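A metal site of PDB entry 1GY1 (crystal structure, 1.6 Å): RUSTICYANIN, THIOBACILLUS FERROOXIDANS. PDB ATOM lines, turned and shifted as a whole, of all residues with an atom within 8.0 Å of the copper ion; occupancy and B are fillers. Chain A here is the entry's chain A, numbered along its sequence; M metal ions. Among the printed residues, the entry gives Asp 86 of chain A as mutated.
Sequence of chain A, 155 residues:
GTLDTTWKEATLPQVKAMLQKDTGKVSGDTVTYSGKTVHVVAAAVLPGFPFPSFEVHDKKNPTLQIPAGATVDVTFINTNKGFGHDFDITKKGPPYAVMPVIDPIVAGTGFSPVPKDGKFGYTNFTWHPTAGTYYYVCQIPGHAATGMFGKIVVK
The backbone carbonyl oxygen (O) of His 85 sits at hydrogen-bond distance from the side-chain hydroxyl (OG) of Ser 112, 2.6 Å away. The side-chain amide nitrogen (ND2) of Asn 80 sits at hydrogen-bond distance from a ring nitrogen (NE2) of His 85, at 2.7 Å. The side-chain carboxylate (OD1) of Asp 86 sits close to the side-chain sulfur (SG) of Cys 138 (3.5 Å). The backbone NH (N) of Ile 140 sits close to the side-chain sulfur (SG) of Cys 138 (3.4 Å). The side-chain hydroxyl (OG1) of Thr 146 is in hydrogen-bond range of the backbone carbonyl oxygen (O) of His 143 (3.2 Å).
Merely in contact with the copper ion: Ile 140. Of the 27 residues printed, 5 come within 4 Å of the copper ion. The nearest printed residue that does not touch the copper ion is Asp 86 (5.0 Å).
The copper ion is bound by a ring nitrogen (ND1) of His 143, a ring nitrogen (ND1) of His 85, the side-chain sulfur of Cys 138 and the side-chain sulfur of Met 148. The copper ion has four donor atoms within binding distance.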
ATOM      1  N   ALA A  44     -13.960 -15.597  21.846  1.00  0.00           N
ATOM      2  CA  ALA A  44     -15.255 -16.190  22.121  1.00  0.00           C
ATOM      3  C   ALA A  44     -16.328 -15.363  21.449  1.00  0.00           C
ATOM      4  O   ALA A  44     -16.482 -14.180  21.757  1.00  0.00           O
ATOM      5  CB  ALA A  44     -15.495 -16.254  23.623  1.00  0.00           C
ATOM      6  N   VAL A  45     -16.996 -15.958  20.469  1.00  0.00           N
ATOM      7  CA  VAL A  45     -18.115 -15.371  19.748  1.00  0.00           C
ATOM      8  C   VAL A  45     -17.833 -13.975  19.201  1.00  0.00           C
ATOM      9  O   VAL A  45     -18.258 -12.953  19.738  1.00  0.00           O
ATOM     10  CB  VAL A  45     -19.419 -15.345  20.606  1.00  0.00           C
ATOM     11  CG1 VAL A  45     -20.641 -14.995  19.712  1.00  0.00           C
ATOM     12  CG2 VAL A  45     -19.644 -16.660  21.319  1.00  0.00           C
ATOM     13  N   PHE A  51     -23.397 -18.190  18.249  1.00  0.00           N
ATOM     14  CA  PHE A  51     -23.235 -18.468  19.658  1.00  0.00           C
ATOM     15  C   PHE A  51     -23.695 -19.910  19.899  1.00  0.00           C
ATOM     16  O   PHE A  51     -24.685 -20.349  19.312  1.00  0.00           O
ATOM     17  CB  PHE A  51     -24.092 -17.483  20.472  1.00  0.00           C
ATOM     18  CG  PHE A  51     -24.196 -17.839  21.906  1.00  0.00           C
ATOM     19  CD1 PHE A  51     -25.047 -18.840  22.326  1.00  0.00           C
ATOM     20  CD2 PHE A  51     -23.411 -17.186  22.853  1.00  0.00           C
ATOM     21  CE1 PHE A  51     -25.108 -19.197  23.653  1.00  0.00           C
ATOM     22  CE2 PHE A  51     -23.500 -17.532  24.182  1.00  0.00           C
ATOM     23  CZ  PHE A  51     -24.351 -18.528  24.571  1.00  0.00           C
ATOM     24  N   PRO A  52     -22.982 -20.695  20.708  1.00  0.00           N
ATOM     25  CA  PRO A  52     -21.694 -20.350  21.294  1.00  0.00           C
ATOM     26  C   PRO A  52     -20.551 -21.013  20.538  1.00  0.00           C
ATOM     27  O   PRO A  52     -20.603 -22.183  20.154  1.00  0.00           O
ATOM     28  CB  PRO A  52     -21.836 -20.901  22.704  1.00  0.00           C
ATOM     29  CG  PRO A  52     -22.597 -22.179  22.502  1.00  0.00           C
ATOM     30  CD  PRO A  52     -23.442 -21.991  21.248  1.00  0.00           C
ATOM     31  N   SER A  53     -19.490 -20.259  20.298  1.00  0.00           N
ATOM     32  CA  SER A  53     -18.373 -20.766  19.508  1.00  0.00           C
ATOM     33  C   SER A  53     -17.136 -19.963  19.787  1.00  0.00           C
ATOM     34  O   SER A  53     -17.189 -18.841  20.292  1.00  0.00           O
ATOM     35  CB  SER A  53     -18.660 -20.639  18.001  1.00  0.00           C
ATOM     36  OG  SER A  53     -18.809 -19.271  17.588  1.00  0.00           O
ATOM     37  N   PHE A  54     -16.010 -20.553  19.441  1.00  0.00           N
ATOM     38  CA  PHE A  54     -14.736 -19.869  19.474  1.00  0.00           C
ATOM     39  C   PHE A  54     -14.345 -19.605  18.031  1.00  0.00           C
ATOM     40  O   PHE A  54     -14.618 -20.424  17.142  1.00  0.00           O
ATOM     41  CB  PHE A  54     -13.618 -20.743  20.034  1.00  0.00           C
ATOM     42  CG  PHE A  54     -13.760 -21.115  21.475  1.00  0.00           C
ATOM     43  CD1 PHE A  54     -13.385 -20.230  22.474  1.00  0.00           C
ATOM     44  CD2 PHE A  54     -14.174 -22.384  21.823  1.00  0.00           C
ATOM     45  CE1 PHE A  54     -13.493 -20.593  23.788  1.00  0.00           C
ATOM     46  CE2 PHE A  54     -14.282 -22.747  23.137  1.00  0.00           C
ATOM     47  CZ  PHE A  54     -13.923 -21.846  24.126  1.00  0.00           C
ATOM     48  N   PHE A  76      -6.231 -15.688  24.419  1.00  0.00           N
ATOM     49  CA  PHE A  76      -7.685 -15.884  24.419  1.00  0.00           C
ATOM     50  C   PHE A  76      -8.346 -14.573  24.774  1.00  0.00           C
ATOM     51  O   PHE A  76      -8.034 -13.961  25.811  1.00  0.00           O
ATOM     52  CB  PHE A  76      -8.104 -16.971  25.408  1.00  0.00           C
ATOM     53  CG  PHE A  76      -9.581 -17.053  25.591  1.00  0.00           C
ATOM     54  CD1 PHE A  76     -10.417 -17.316  24.517  1.00  0.00           C
ATOM     55  CD2 PHE A  76     -10.136 -16.842  26.833  1.00  0.00           C
ATOM     56  CE1 PHE A  76     -11.771 -17.360  24.689  1.00  0.00           C
ATOM     57  CE2 PHE A  76     -11.497 -16.905  27.008  1.00  0.00           C
ATOM     58  CZ  PHE A  76     -12.313 -17.144  25.929  1.00  0.00           C
ATOM     59  N   ASN A  78     -12.108 -12.545  25.217  1.00  0.00           N
ATOM     60  CA  ASN A  78     -13.541 -12.725  25.364  1.00  0.00           C
ATOM     61  C   ASN A  78     -14.231 -11.492  24.838  1.00  0.00           C
ATOM     62  O   ASN A  78     -14.297 -10.475  25.529  1.00  0.00           O
ATOM     63  CB  ASN A  78     -13.969 -12.998  26.804  1.00  0.00           C
ATOM     64  CG  ASN A  78     -15.489 -13.094  26.934  1.00  0.00           C
ATOM     65  OD1 ASN A  78     -16.047 -12.938  28.030  1.00  0.00           O
ATOM     66  ND2 ASN A  78     -16.137 -13.375  25.856  1.00  0.00           N
ATOM     67  N   ASN A  80     -17.432 -11.538  23.805  1.00  0.00           N
ATOM     68  CA  ASN A  80     -18.861 -11.791  23.848  1.00  0.00           C
ATOM     69  C   ASN A  80     -19.585 -11.148  25.005  1.00  0.00           C
ATOM     70  O   ASN A  80     -19.510 -11.602  26.131  1.00  0.00           O
ATOM     71  CB  ASN A  80     -19.094 -13.297  23.902  1.00  0.00           C
ATOM     72  CG  ASN A  80     -20.514 -13.698  23.523  1.00  0.00           C
ATOM     73  OD1 ASN A  80     -21.251 -12.966  22.804  1.00  0.00           O
ATOM     74  ND2 ASN A  80     -20.892 -14.871  23.947  1.00  0.00           N
ATOM     75  N   PHE A  83     -21.260 -12.722  28.750  1.00  0.00           N
ATOM     76  CA  PHE A  83     -20.753 -14.027  29.136  1.00  0.00           C
ATOM     77  C   PHE A  83     -19.292 -13.939  29.554  1.00  0.00           C
ATOM     78  O   PHE A  83     -18.550 -13.105  29.045  1.00  0.00           O
ATOM     79  CB  PHE A  83     -20.879 -15.004  27.961  1.00  0.00           C
ATOM     80  CG  PHE A  83     -22.288 -15.226  27.510  1.00  0.00           C
ATOM     81  CD1 PHE A  83     -22.821 -14.433  26.513  1.00  0.00           C
ATOM     82  CD2 PHE A  83     -23.062 -16.210  28.090  1.00  0.00           C
ATOM     83  CE1 PHE A  83     -24.124 -14.615  26.094  1.00  0.00           C
ATOM     84  CE2 PHE A  83     -24.369 -16.400  27.673  1.00  0.00           C
ATOM     85  CZ  PHE A  83     -24.894 -15.613  26.665  1.00  0.00           C
ATOM     86  N   GLY A  84     -18.892 -14.801  30.476  1.00  0.00           N
ATOM     87  CA  GLY A  84     -17.494 -14.870  30.909  1.00  0.00           C
ATOM     88  C   GLY A  84     -16.879 -16.211  30.533  1.00  0.00           C
ATOM     89  O   GLY A  84     -16.449 -16.986  31.390  1.00  0.00           O
ATOM     90  N   HIS A  85     -16.783 -16.448  29.235  1.00  0.00           N
ATOM     91  CA  HIS A  85     -16.298 -17.728  28.719  1.00  0.00           C
ATOM     92  C   HIS A  85     -14.888 -18.039  29.166  1.00  0.00           C
ATOM     93  O   HIS A  85     -14.107 -17.128  29.426  1.00  0.00           O
ATOM     94  CB  HIS A  85     -16.256 -17.698  27.207  1.00  0.00           C
ATOM     95  CG  HIS A  85     -17.554 -17.325  26.544  1.00  0.00           C
ATOM     96  ND1 HIS A  85     -18.551 -18.237  26.294  1.00  0.00           N
ATOM     97  CD2 HIS A  85     -17.941 -16.162  25.973  1.00  0.00           C
ATOM     98  CE1 HIS A  85     -19.531 -17.640  25.634  1.00  0.00           C
ATOM     99  NE2 HIS A  85     -19.191 -16.372  25.438  1.00  0.00           N
ATOM    100  N   ASP A  86     -14.580 -19.314  29.262  1.00  0.00           N
ATOM    101  CA  ASP A  86     -13.205 -19.719  29.512  1.00  0.00           C
ATOM    102  C   ASP A  86     -12.679 -20.461  28.271  1.00  0.00           C
ATOM    103  O   ASP A  86     -13.390 -20.680  27.296  1.00  0.00           O
ATOM    104  CB  ASP A  86     -13.052 -20.533  30.808  1.00  0.00           C
ATOM    105  CG  ASP A  86     -13.921 -21.768  30.880  1.00  0.00           C
ATOM    106  OD1 ASP A  86     -14.600 -22.096  29.913  1.00  0.00           O
ATOM    107  OD2 ASP A  86     -13.959 -22.484  31.928  1.00  0.00           O
ATOM    108  N   PHE A  87     -11.396 -20.801  28.302  1.00  0.00           N
ATOM    109  CA  PHE A  87     -10.740 -21.494  27.200  1.00  0.00           C
ATOM    110  C   PHE A  87      -9.841 -22.536  27.869  1.00  0.00           C
ATOM    111  O   PHE A  87      -8.795 -22.190  28.418  1.00  0.00           O
ATOM    112  CB  PHE A  87      -9.927 -20.531  26.323  1.00  0.00           C
ATOM    113  CG  PHE A  87      -9.288 -21.159  25.114  1.00  0.00           C
ATOM    114  CD1 PHE A  87      -9.864 -21.085  23.866  1.00  0.00           C
ATOM    115  CD2 PHE A  87      -8.082 -21.822  25.243  1.00  0.00           C
ATOM    116  CE1 PHE A  87      -9.227 -21.663  22.764  1.00  0.00           C
ATOM    117  CE2 PHE A  87      -7.454 -22.419  24.134  1.00  0.00           C
ATOM    118  CZ  PHE A  87      -8.027 -22.320  22.913  1.00  0.00           C
ATOM    119  N   PHE A 111     -12.634 -18.452  34.260  1.00  0.00           N
ATOM    120  CA  PHE A 111     -13.667 -17.710  33.561  1.00  0.00           C
ATOM    121  C   PHE A 111     -13.208 -16.275  33.341  1.00  0.00           C
ATOM    122  O   PHE A 111     -12.623 -15.651  34.238  1.00  0.00           O
ATOM    123  CB  PHE A 111     -14.977 -17.760  34.337  1.00  0.00           C
ATOM    124  CG  PHE A 111     -15.558 -19.139  34.415  1.00  0.00           C
ATOM    125  CD1 PHE A 111     -16.009 -19.778  33.278  1.00  0.00           C
ATOM    126  CD2 PHE A 111     -15.638 -19.811  35.627  1.00  0.00           C
ATOM    127  CE1 PHE A 111     -16.567 -21.047  33.352  1.00  0.00           C
ATOM    128  CE2 PHE A 111     -16.177 -21.087  35.698  1.00  0.00           C
ATOM    129  CZ  PHE A 111     -16.631 -21.704  34.559  1.00  0.00           C
ATOM    130  N   SER A 112     -13.474 -15.769  32.155  1.00  0.00           N
ATOM    131  CA  SER A 112     -13.089 -14.412  31.812  1.00  0.00           C
ATOM    132  C   SER A 112     -14.092 -13.403  32.359  1.00  0.00           C
ATOM    133  O   SER A 112     -15.232 -13.725  32.664  1.00  0.00           O
ATOM    134  CB  SER A 112     -12.998 -14.259  30.300  1.00  0.00           C
ATOM    135  OG  SER A 112     -14.253 -14.544  29.693  1.00  0.00           O
ATOM    136  N   VAL A 137     -12.277 -26.072  25.069  1.00  0.00           N
ATOM    137  CA  VAL A 137     -13.650 -26.149  25.532  1.00  0.00           C
ATOM    138  C   VAL A 137     -13.959 -25.011  26.456  1.00  0.00           C
ATOM    139  O   VAL A 137     -13.077 -24.521  27.164  1.00  0.00           O
ATOM    140  CB  VAL A 137     -13.837 -27.475  26.332  1.00  0.00           C
ATOM    141  CG1 VAL A 137     -15.281 -27.700  26.780  1.00  0.00           C
ATOM    142  CG2 VAL A 137     -13.387 -28.663  25.505  1.00  0.00           C
ATOM    143  N   CYS A 138     -15.222 -24.569  26.431  1.00  0.00           N
ATOM    144  CA  CYS A 138     -15.725 -23.629  27.413  1.00  0.00           C
ATOM    145  C   CYS A 138     -16.519 -24.422  28.453  1.00  0.00           C
ATOM    146  O   CYS A 138     -17.264 -25.353  28.089  1.00  0.00           O
ATOM    147  CB  CYS A 138     -16.626 -22.595  26.756  1.00  0.00           C
ATOM    148  SG  CYS A 138     -17.353 -21.428  27.938  1.00  0.00           S
ATOM    149  N   GLN A 139     -16.349 -24.086  29.723  1.00  0.00           N
ATOM    150  CA  GLN A 139     -17.036 -24.782  30.808  1.00  0.00           C
ATOM    151  C   GLN A 139     -18.277 -24.041  31.346  1.00  0.00           C
ATOM    152  O   GLN A 139     -18.902 -24.507  32.326  1.00  0.00           O
ATOM    153  CB  GLN A 139     -16.084 -25.059  31.975  1.00  0.00           C
ATOM    154  CG  GLN A 139     -14.876 -25.905  31.646  1.00  0.00           C
ATOM    155  CD  GLN A 139     -14.078 -26.236  32.912  1.00  0.00           C
ATOM    156  OE1 GLN A 139     -13.102 -25.554  33.230  1.00  0.00           O
ATOM    157  NE2 GLN A 139     -14.558 -27.199  33.652  1.00  0.00           N
ATOM    158  N   ILE A 140     -18.644 -22.908  30.766  1.00  0.00           N
ATOM    159  CA  ILE A 140     -19.883 -22.247  31.211  1.00  0.00           C
ATOM    160  C   ILE A 140     -20.984 -23.259  30.976  1.00  0.00           C
ATOM    161  O   ILE A 140     -21.109 -23.768  29.881  1.00  0.00           O
ATOM    162  CB  ILE A 140     -20.190 -20.973  30.445  1.00  0.00           C
ATOM    163  CG1 ILE A 140     -19.137 -19.903  30.730  1.00  0.00           C
ATOM    164  CG2 ILE A 140     -21.596 -20.521  30.814  1.00  0.00           C
ATOM    165  CD1 ILE A 140     -19.433 -18.567  30.037  1.00  0.00           C
ATOM    166  N   PRO A 141     -21.784 -23.576  31.985  1.00  0.00           N
ATOM    167  CA  PRO A 141     -22.789 -24.611  31.831  1.00  0.00           C
ATOM    168  C   PRO A 141     -23.606 -24.482  30.549  1.00  0.00           C
ATOM    169  O   PRO A 141     -24.171 -23.423  30.248  1.00  0.00           O
ATOM    170  CB  PRO A 141     -23.653 -24.443  33.080  1.00  0.00           C
ATOM    171  CG  PRO A 141     -22.665 -24.000  34.083  1.00  0.00           C
ATOM    172  CD  PRO A 141     -21.780 -23.029  33.357  1.00  0.00           C
ATOM    173  N   GLY A 142     -23.616 -25.566  29.795  1.00  0.00           N
ATOM    174  CA  GLY A 142     -24.349 -25.700  28.561  1.00  0.00           C
ATOM    175  C   GLY A 142     -23.628 -25.328  27.293  1.00  0.00           C
ATOM    176  O   GLY A 142     -24.043 -25.726  26.196  1.00  0.00           O
ATOM    177  N   HIS A 143     -22.535 -24.580  27.426  1.00  0.00           N
ATOM    178  CA  HIS A 143     -21.876 -24.032  26.229  1.00  0.00           C
ATOM    179  C   HIS A 143     -21.229 -25.127  25.375  1.00  0.00           C
ATOM    180  O   HIS A 143     -21.462 -25.209  24.177  1.00  0.00           O
ATOM    181  CB  HIS A 143     -20.865 -22.953  26.601  1.00  0.00           C
ATOM    182  CG  HIS A 143     -21.505 -21.660  27.026  1.00  0.00           C
ATOM    183  ND1 HIS A 143     -20.856 -20.443  26.986  1.00  0.00           N
ATOM    184  CD2 HIS A 143     -22.752 -21.397  27.475  1.00  0.00           C
ATOM    185  CE1 HIS A 143     -21.667 -19.494  27.422  1.00  0.00           C
ATOM    186  NE2 HIS A 143     -22.824 -20.049  27.724  1.00  0.00           N
ATOM    187  N   ALA A 144     -20.428 -25.974  26.006  1.00  0.00           N
ATOM    188  CA  ALA A 144     -19.781 -27.071  25.274  1.00  0.00           C
ATOM    189  C   ALA A 144     -20.825 -28.033  24.742  1.00  0.00           C
ATOM    190  O   ALA A 144     -20.684 -28.550  23.631  1.00  0.00           O
ATOM    191  CB  ALA A 144     -18.798 -27.789  26.130  1.00  0.00           C
ATOM    192  N   THR A 146     -23.595 -27.338  23.619  1.00  0.00           N
ATOM    193  CA  THR A 146     -24.266 -26.744  22.469  1.00  0.00           C
ATOM    194  C   THR A 146     -23.282 -26.280  21.399  1.00  0.00           C
ATOM    195  O   THR A 146     -23.628 -25.460  20.545  1.00  0.00           O
ATOM    196  CB  THR A 146     -25.227 -25.624  22.866  1.00  0.00           C
ATOM    197  OG1 THR A 146     -24.598 -24.666  23.721  1.00  0.00           O
ATOM    198  CG2 THR A 146     -26.392 -26.187  23.698  1.00  0.00           C
ATOM    199  N   MET A 148     -19.693 -25.194  21.879  1.00  0.00           N
ATOM    200  CA  MET A 148     -18.546 -24.316  22.142  1.00  0.00           C
ATOM    201  C   MET A 148     -17.269 -25.092  22.476  1.00  0.00           C
ATOM    202  O   MET A 148     -16.835 -25.172  23.623  1.00  0.00           O
ATOM    203  CB  MET A 148     -18.862 -23.282  23.211  1.00  0.00           C
ATOM    204  CG  MET A 148     -17.842 -22.171  23.202  1.00  0.00           C
ATOM    205  SD  MET A 148     -18.403 -20.706  24.075  1.00  0.00           S
ATOM    206  CE  MET A 148     -16.921 -19.663  23.746  1.00  0.00           C
ATOM    207  N   PHE A 149     -16.665 -25.658  21.439  1.00  0.00           N
ATOM    208  CA  PHE A 149     -15.441 -26.407  21.543  1.00  0.00           C
ATOM    209  C   PHE A 149     -14.919 -26.633  20.135  1.00  0.00           C
ATOM    210  O   PHE A 149     -15.648 -26.520  19.157  1.00  0.00           O
ATOM    211  CB  PHE A 149     -15.669 -27.774  22.201  1.00  0.00           C
ATOM    212  CG  PHE A 149     -16.514 -28.709  21.374  1.00  0.00           C
ATOM    213  CD1 PHE A 149     -17.885 -28.768  21.550  1.00  0.00           C
ATOM    214  CD2 PHE A 149     -15.916 -29.565  20.471  1.00  0.00           C
ATOM    215  CE1 PHE A 149     -18.637 -29.652  20.796  1.00  0.00           C
ATOM    216  CE2 PHE A 149     -16.668 -30.424  19.734  1.00  0.00           C
ATOM    217  CZ  PHE A 149     -18.014 -30.473  19.896  1.00  0.00           C
HETATM  218 CU    CU M   1     -18.802 -20.264  26.773  1.00  0.00          CU
